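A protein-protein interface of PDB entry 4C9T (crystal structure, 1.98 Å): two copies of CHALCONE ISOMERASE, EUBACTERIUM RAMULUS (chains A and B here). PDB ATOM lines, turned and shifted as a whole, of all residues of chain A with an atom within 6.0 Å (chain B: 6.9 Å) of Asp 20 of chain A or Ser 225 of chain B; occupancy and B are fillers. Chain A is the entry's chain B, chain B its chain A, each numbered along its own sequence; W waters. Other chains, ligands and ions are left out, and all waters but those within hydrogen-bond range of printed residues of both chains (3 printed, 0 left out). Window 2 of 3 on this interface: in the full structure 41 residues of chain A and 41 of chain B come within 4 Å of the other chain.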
ATOM      1  N   SER A  18     -24.107 -30.283   0.895  1.00  0.00           N
ATOM      2  CA  SER A  18     -23.446 -29.013   1.191  1.00  0.00           C
ATOM      3  C   SER A  18     -24.329 -28.247   2.147  1.00  0.00           C
ATOM      4  O   SER A  18     -25.549 -28.267   2.014  1.00  0.00           O
ATOM      5  CB  SER A  18     -23.187 -28.142  -0.071  1.00  0.00           C
ATOM      6  OG  SER A  18     -22.924 -26.778   0.287  1.00  0.00           O
ATOM      7  N   GLU A  19     -23.718 -27.515   3.076  1.00  0.00           N
ATOM      8  CA  GLU A  19     -24.491 -26.723   4.039  1.00  0.00           C
ATOM      9  C   GLU A  19     -25.276 -25.654   3.343  1.00  0.00           C
ATOM     10  O   GLU A  19     -26.359 -25.242   3.792  1.00  0.00           O
ATOM     11  CB  GLU A  19     -23.604 -26.184   5.170  1.00  0.00           C
ATOM     12  CG  GLU A  19     -23.172 -27.296   6.111  1.00  0.00           C
ATOM     13  CD  GLU A  19     -24.381 -28.036   6.755  1.00  0.00           C
ATOM     14  OE1 GLU A  19     -25.344 -27.384   7.210  1.00  0.00           O
ATOM     15  OE2 GLU A  19     -24.412 -29.298   6.678  1.00  0.00           O
ATOM     16  N   ASP A  20     -24.820 -25.250   2.178  1.00  0.00           N
ATOM     17  CA  ASP A  20     -25.567 -24.253   1.474  1.00  0.00           C
ATOM     18  C   ASP A  20     -26.931 -24.718   0.992  1.00  0.00           C
ATOM     19  O   ASP A  20     -27.780 -23.903   0.691  1.00  0.00           O
ATOM     20  CB  ASP A  20     -24.745 -23.641   0.341  1.00  0.00           C
ATOM     21  CG  ASP A  20     -23.657 -22.670   0.898  1.00  0.00           C
ATOM     22  OD1 ASP A  20     -23.729 -22.164   2.083  1.00  0.00           O
ATOM     23  OD2 ASP A  20     -22.702 -22.434   0.163  1.00  0.00           O
ATOM     24  N   TYR A  21     -27.104 -26.026   0.855  1.00  0.00           N
ATOM     25  CA  TYR A  21     -28.356 -26.541   0.417  1.00  0.00           C
ATOM     26  C   TYR A  21     -29.344 -26.783   1.579  1.00  0.00           C
ATOM     27  O   TYR A  21     -30.528 -27.056   1.321  1.00  0.00           O
ATOM     28  CB  TYR A  21     -28.126 -27.859  -0.310  1.00  0.00           C
ATOM     29  CG  TYR A  21     -27.308 -27.810  -1.559  1.00  0.00           C
ATOM     30  CD1 TYR A  21     -27.275 -26.688  -2.349  1.00  0.00           C
ATOM     31  CD2 TYR A  21     -26.603 -28.952  -1.967  1.00  0.00           C
ATOM     32  CE1 TYR A  21     -26.532 -26.665  -3.555  1.00  0.00           C
ATOM     33  CE2 TYR A  21     -25.888 -28.971  -3.136  1.00  0.00           C
ATOM     34  CZ  TYR A  21     -25.858 -27.835  -3.924  1.00  0.00           C
ATOM     35  OH  TYR A  21     -25.150 -27.862  -5.062  1.00  0.00           O
ATOM     36  N   ARG A  22     -28.877 -26.727   2.807  1.00  0.00           N
ATOM     37  CA  ARG A  22     -29.694 -27.100   3.971  1.00  0.00           C
ATOM     38  C   ARG A  22     -31.010 -26.357   4.095  1.00  0.00           C
ATOM     39  O   ARG A  22     -32.051 -27.013   4.201  1.00  0.00           O
ATOM     40  CB  ARG A  22     -28.884 -27.081   5.288  1.00  0.00           C
ATOM     41  CG  ARG A  22     -29.662 -27.664   6.481  1.00  0.00           C
ATOM     42  CD  ARG A  22     -28.837 -27.681   7.771  1.00  0.00           C
ATOM     43  NE  ARG A  22     -27.737 -28.583   7.602  1.00  0.00           N
ATOM     44  CZ  ARG A  22     -27.837 -29.910   7.792  1.00  0.00           C
ATOM     45  NH1 ARG A  22     -28.946 -30.472   8.244  1.00  0.00           N
ATOM     46  NH2 ARG A  22     -26.806 -30.663   7.545  1.00  0.00           N
ATOM     47  N   PRO A  23     -31.026 -25.024   3.953  1.00  0.00           N
ATOM     48  CA  PRO A  23     -32.308 -24.318   4.112  1.00  0.00           C
ATOM     49  C   PRO A  23     -33.313 -24.698   3.009  1.00  0.00           C
ATOM     50  O   PRO A  23     -34.494 -24.854   3.257  1.00  0.00           O
ATOM     51  CB  PRO A  23     -31.888 -22.833   4.075  1.00  0.00           C
ATOM     52  CG  PRO A  23     -30.428 -22.796   4.502  1.00  0.00           C
ATOM     53  CD  PRO A  23     -29.880 -24.070   3.906  1.00  0.00           C
ATOM     54  N   LYS A  24     -32.824 -24.900   1.809  1.00  0.00           N
ATOM     55  CA  LYS A  24     -33.684 -25.238   0.713  1.00  0.00           C
ATOM     56  C   LYS A  24     -34.258 -26.653   0.815  1.00  0.00           C
ATOM     57  O   LYS A  24     -35.442 -26.856   0.592  1.00  0.00           O
ATOM     58  CB  LYS A  24     -32.973 -25.104  -0.624  1.00  0.00           C
ATOM     59  CG  LYS A  24     -32.771 -23.655  -1.093  1.00  0.00           C
ATOM     60  CD  LYS A  24     -31.771 -23.605  -2.285  1.00  0.00           C
ATOM     61  CE  LYS A  24     -31.700 -22.188  -2.850  1.00  0.00           C
ATOM     62  NZ  LYS A  24     -30.984 -21.367  -1.849  1.00  0.00           N
ATOM     63  N   TYR B 161     -31.941 -18.373   5.753  1.00  0.00           N
ATOM     64  CA  TYR B 161     -30.939 -18.666   6.785  1.00  0.00           C
ATOM     65  C   TYR B 161     -30.982 -17.491   7.724  1.00  0.00           C
ATOM     66  O   TYR B 161     -30.438 -16.427   7.428  1.00  0.00           O
ATOM     67  CB  TYR B 161     -29.565 -18.858   6.131  1.00  0.00           C
ATOM     68  CG  TYR B 161     -28.423 -19.275   7.045  1.00  0.00           C
ATOM     69  CD1 TYR B 161     -27.619 -18.340   7.642  1.00  0.00           C
ATOM     70  CD2 TYR B 161     -28.074 -20.600   7.194  1.00  0.00           C
ATOM     71  CE1 TYR B 161     -26.533 -18.722   8.436  1.00  0.00           C
ATOM     72  CE2 TYR B 161     -26.985 -20.992   7.959  1.00  0.00           C
ATOM     73  CZ  TYR B 161     -26.223 -20.043   8.582  1.00  0.00           C
ATOM     74  OH  TYR B 161     -25.157 -20.454   9.343  1.00  0.00           O
ATOM     75  N   GLU B 195     -26.191 -10.416  -0.518  1.00  0.00           N
ATOM     76  CA  GLU B 195     -26.358 -11.717   0.094  1.00  0.00           C
ATOM     77  C   GLU B 195     -27.349 -11.626   1.299  1.00  0.00           C
ATOM     78  O   GLU B 195     -27.834 -12.657   1.767  1.00  0.00           O
ATOM     79  CB  GLU B 195     -25.032 -12.181   0.656  1.00  0.00           C
ATOM     80  CG  GLU B 195     -23.998 -12.497  -0.433  1.00  0.00           C
ATOM     81  CD  GLU B 195     -23.246 -11.258  -0.949  1.00  0.00           C
ATOM     82  OE1 GLU B 195     -23.390 -10.126  -0.393  1.00  0.00           O
ATOM     83  OE2 GLU B 195     -22.473 -11.484  -1.900  1.00  0.00           O
ATOM     84  N   PHE B 221     -29.916 -14.490   5.381  1.00  0.00           N
ATOM     85  CA  PHE B 221     -29.109 -14.839   4.235  1.00  0.00           C
ATOM     86  C   PHE B 221     -29.731 -16.008   3.502  1.00  0.00           C
ATOM     87  O   PHE B 221     -30.710 -16.575   3.926  1.00  0.00           O
ATOM     88  CB  PHE B 221     -27.715 -15.255   4.715  1.00  0.00           C
ATOM     89  CG  PHE B 221     -27.025 -14.170   5.494  1.00  0.00           C
ATOM     90  CD1 PHE B 221     -26.353 -13.161   4.827  1.00  0.00           C
ATOM     91  CD2 PHE B 221     -27.130 -14.107   6.865  1.00  0.00           C
ATOM     92  CE1 PHE B 221     -25.785 -12.103   5.517  1.00  0.00           C
ATOM     93  CE2 PHE B 221     -26.539 -13.111   7.570  1.00  0.00           C
ATOM     94  CZ  PHE B 221     -25.860 -12.067   6.892  1.00  0.00           C
ATOM     95  N   GLU B 222     -29.188 -16.335   2.340  1.00  0.00           N
ATOM     96  CA  GLU B 222     -29.615 -17.488   1.605  1.00  0.00           C
ATOM     97  C   GLU B 222     -29.044 -18.747   2.219  1.00  0.00           C
ATOM     98  O   GLU B 222     -29.668 -19.814   2.171  1.00  0.00           O
ATOM     99  CB  GLU B 222     -29.174 -17.331   0.139  1.00  0.00           C
ATOM    100  CG  GLU B 222     -29.745 -18.391  -0.722  1.00  0.00           C
ATOM    101  CD  GLU B 222     -29.358 -18.230  -2.232  1.00  0.00           C
ATOM    102  OE1 GLU B 222     -28.500 -17.388  -2.526  1.00  0.00           O
ATOM    103  OE2 GLU B 222     -29.942 -18.965  -3.066  1.00  0.00           O
ATOM    104  N   ASN B 223     -27.884 -18.612   2.832  1.00  0.00           N
ATOM    105  CA  ASN B 223     -27.084 -19.760   3.260  1.00  0.00           C
ATOM    106  C   ASN B 223     -25.875 -19.384   4.044  1.00  0.00           C
ATOM    107  O   ASN B 223     -25.536 -18.219   4.230  1.00  0.00           O
ATOM    108  CB  ASN B 223     -26.639 -20.640   2.101  1.00  0.00           C
ATOM    109  CG  ASN B 223     -25.954 -19.867   1.029  1.00  0.00           C
ATOM    110  OD1 ASN B 223     -25.074 -19.037   1.304  1.00  0.00           O
ATOM    111  ND2 ASN B 223     -26.408 -20.067  -0.204  1.00  0.00           N
ATOM    112  N   GLN B 224     -25.269 -20.402   4.607  1.00  0.00           N
ATOM    113  CA  GLN B 224     -24.077 -20.230   5.404  1.00  0.00           C
ATOM    114  C   GLN B 224     -22.969 -19.469   4.664  1.00  0.00           C
ATOM    115  O   GLN B 224     -22.281 -18.659   5.287  1.00  0.00           O
ATOM    116  CB  GLN B 224     -23.563 -21.611   5.775  1.00  0.00           C
ATOM    117  CG  GLN B 224     -22.318 -21.594   6.574  1.00  0.00           C
ATOM    118  CD  GLN B 224     -21.838 -22.995   6.894  1.00  0.00           C
ATOM    119  OE1 GLN B 224     -22.271 -23.608   7.871  1.00  0.00           O
ATOM    120  NE2 GLN B 224     -20.931 -23.506   6.069  1.00  0.00           N
ATOM    121  N   SER B 225     -22.766 -19.733   3.376  1.00  0.00           N
ATOM    122  CA  SER B 225     -21.686 -19.009   2.613  1.00  0.00           C
ATOM    123  C   SER B 225     -21.971 -17.524   2.564  1.00  0.00           C
ATOM    124  O   SER B 225     -21.079 -16.699   2.749  1.00  0.00           O
ATOM    125  CB  SER B 225     -21.538 -19.536   1.168  1.00  0.00           C
ATOM    126  OG  SER B 225     -20.992 -20.806   1.297  1.00  0.00           O
ATOM    127  N   GLY B 226     -23.243 -17.196   2.403  1.00  0.00           N
ATOM    128  CA  GLY B 226     -23.682 -15.786   2.462  1.00  0.00           C
ATOM    129  C   GLY B 226     -23.460 -15.115   3.801  1.00  0.00           C
ATOM    130  O   GLY B 226     -22.938 -13.993   3.859  1.00  0.00           O
ATOM    131  N   TRP B 227     -23.833 -15.812   4.882  1.00  0.00           N
ATOM    132  CA  TRP B 227     -23.577 -15.348   6.242  1.00  0.00           C
ATOM    133  C   TRP B 227     -22.075 -15.042   6.434  1.00  0.00           C
ATOM    134  O   TRP B 227     -21.686 -13.964   6.941  1.00  0.00           O
ATOM    135  CB  TRP B 227     -24.037 -16.421   7.234  1.00  0.00           C
ATOM    136  CG  TRP B 227     -23.671 -16.082   8.646  1.00  0.00           C
ATOM    137  CD1 TRP B 227     -24.430 -15.359   9.535  1.00  0.00           C
ATOM    138  CD2 TRP B 227     -22.435 -16.384   9.349  1.00  0.00           C
ATOM    139  NE1 TRP B 227     -23.735 -15.119  10.696  1.00  0.00           N
ATOM    140  CE2 TRP B 227     -22.544 -15.778  10.663  1.00  0.00           C
ATOM    141  CE3 TRP B 227     -21.275 -17.077   9.034  1.00  0.00           C
ATOM    142  CZ2 TRP B 227     -21.539 -15.861  11.593  1.00  0.00           C
ATOM    143  CZ3 TRP B 227     -20.286 -17.180  10.003  1.00  0.00           C
ATOM    144  CH2 TRP B 227     -20.418 -16.571  11.249  1.00  0.00           C
ATOM    145  N   TYR B 228     -21.225 -15.987   6.034  1.00  0.00           N
ATOM    146  CA  TYR B 228     -19.769 -15.850   6.221  1.00  0.00           C
ATOM    147  C   TYR B 228     -19.266 -14.672   5.397  1.00  0.00           C
ATOM    148  O   TYR B 228     -18.553 -13.814   5.903  1.00  0.00           O
ATOM    149  CB  TYR B 228     -19.040 -17.116   5.836  1.00  0.00           C
ATOM    150  CG  TYR B 228     -17.561 -17.068   6.095  1.00  0.00           C
ATOM    151  CD1 TYR B 228     -16.700 -16.466   5.184  1.00  0.00           C
ATOM    152  CD2 TYR B 228     -17.031 -17.592   7.244  1.00  0.00           C
ATOM    153  CE1 TYR B 228     -15.353 -16.412   5.408  1.00  0.00           C
ATOM    154  CE2 TYR B 228     -15.676 -17.548   7.488  1.00  0.00           C
ATOM    155  CZ  TYR B 228     -14.861 -16.954   6.558  1.00  0.00           C
ATOM    156  OH  TYR B 228     -13.559 -16.860   6.822  1.00  0.00           O
ATOM    157  N   LYS B 229     -19.674 -14.608   4.137  1.00  0.00           N
ATOM    158  CA  LYS B 229     -19.241 -13.498   3.285  1.00  0.00           C
ATOM    159  C   LYS B 229     -19.500 -12.134   3.903  1.00  0.00           C
ATOM    160  O   LYS B 229     -18.610 -11.270   3.879  1.00  0.00           O
ATOM    161  CB  LYS B 229     -19.877 -13.570   1.903  1.00  0.00           C
ATOM    162  CG  LYS B 229     -19.389 -12.498   0.912  1.00  0.00           C
ATOM    163  CD  LYS B 229     -20.300 -11.291   0.969  1.00  0.00           C
ATOM    164  CE  LYS B 229     -19.969 -10.217  -0.140  1.00  0.00           C
ATOM    165  NZ  LYS B 229     -20.928  -9.038  -0.014  1.00  0.00           N
ATOM    166  N   VAL B 230     -20.681 -11.951   4.509  1.00  0.00           N
ATOM    167  CA  VAL B 230     -21.048 -10.671   5.093  1.00  0.00           C
ATOM    168  C   VAL B 230     -20.518 -10.487   6.492  1.00  0.00           C
ATOM    169  O   VAL B 230     -19.888  -9.483   6.767  1.00  0.00           O
ATOM    170  CB  VAL B 230     -22.582 -10.480   5.091  1.00  0.00           C
ATOM    171  CG1 VAL B 230     -22.986  -9.109   5.577  1.00  0.00           C
ATOM    172  CG2 VAL B 230     -23.046 -10.606   3.664  1.00  0.00           C
HETATM  173  O   HOH W   1     -26.779 -22.860   4.875  1.00  0.00           O
HETATM  174  O   HOH W   2     -31.771 -20.770   0.791  1.00  0.00           O
HETATM  175  O   HOH W   3     -28.418 -22.025  -1.226  1.00  0.00           O
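Of the 7 printed residues of chain A, 4 touch a printed residue of chain B. Among the printed residues, Asp or Glu carboxylates within 4 Å of a Lys or Arg side-chain nitrogen of the other chain: Lys 24 of chain A with Glu 222 of chain B (2.9 Å).
Water W1 lies within hydrogen-bond range of the backbone carbonyl oxygen (O) of Glu 19 of chain A (2.7 Å) and the backbone NH (N) of Gln 224 of chain B (2.9 Å). Water W2 lies within hydrogen-bond range of the backbone carbonyl oxygen of Glu 222 of chain B (2.7 Å) and the side-chain amino group of Lys 24 of chain A (2.8 Å). Water W3 lies within hydrogen-bond range of the side-chain amino group (NZ) of Lys 24 of chain A, the backbone carbonyl oxygen (O) of Asp 20 of chain A and the side-chain amide nitrogen (ND2) of Asn 223 of chain B.
The side-chain carboxylate of Glu 222 of chain B lies within salt-bridge range of the side-chain amino group of Lys 24 of chain A, 2.9 Å away. OD1 of Asn 223 of chain B lies close to OD1 of Asp 20 of chain A (3.5 Å). The side-chain carboxylate (OD1) of Asp 20 of chain A lies within hydrogen-bond range of the backbone NH (N) of Gln 224 of chain B (3.4 Å). The side-chain carboxylate of Asp 20 of chain A is in hydrogen-bond range of the side-chain hydroxyl of Ser 225 of chain B (2.6 Å).
Printed residues of chain B within 4 Å of Asp 20 of chain A: Asn 223, Gln 224 and Ser 225. Of the printed residues of chain B, Lys 24 of chain A touches Glu 222. Of the printed residues of chain A, Glu 222 of chain B touches Pro 23 (3.9 Å) and Lys 24 (2.9 Å). Of the printed residues of chain A, Asn 223 of chain B touches Asp 20. Ser 225 of chain B touches one residue of chain A. The nearest printed residue of chain B that does not touch Pro 23 of chain A is Tyr 161 of chain B (4.2 Å).
Gln 224 of chain B touches Glu 19 of chain A (NE2 to CB, 3.9 Å). Glu 222 of chain B touches Pro 23 of chain A (O to CG, 3.9 Å).
N of Ser 225 of chain B sits at hydrogen-bond distance from OD1 of Asn 223 of chain B, at 3.2 Å. OD1 of Asn 223 of chain B lies within hydrogen-bond range of N of Gly 226 of chain B (2.8 Å). The side-chain hydroxyl (OG) of Ser 18 of chain A lies close to the backbone NH (N) of Asp 20 of chain A. OE1 of Glu 19 of chain A is in salt-bridge range of NE of Arg 22 of chain A (2.7 Å).
No position is printed for both chains.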
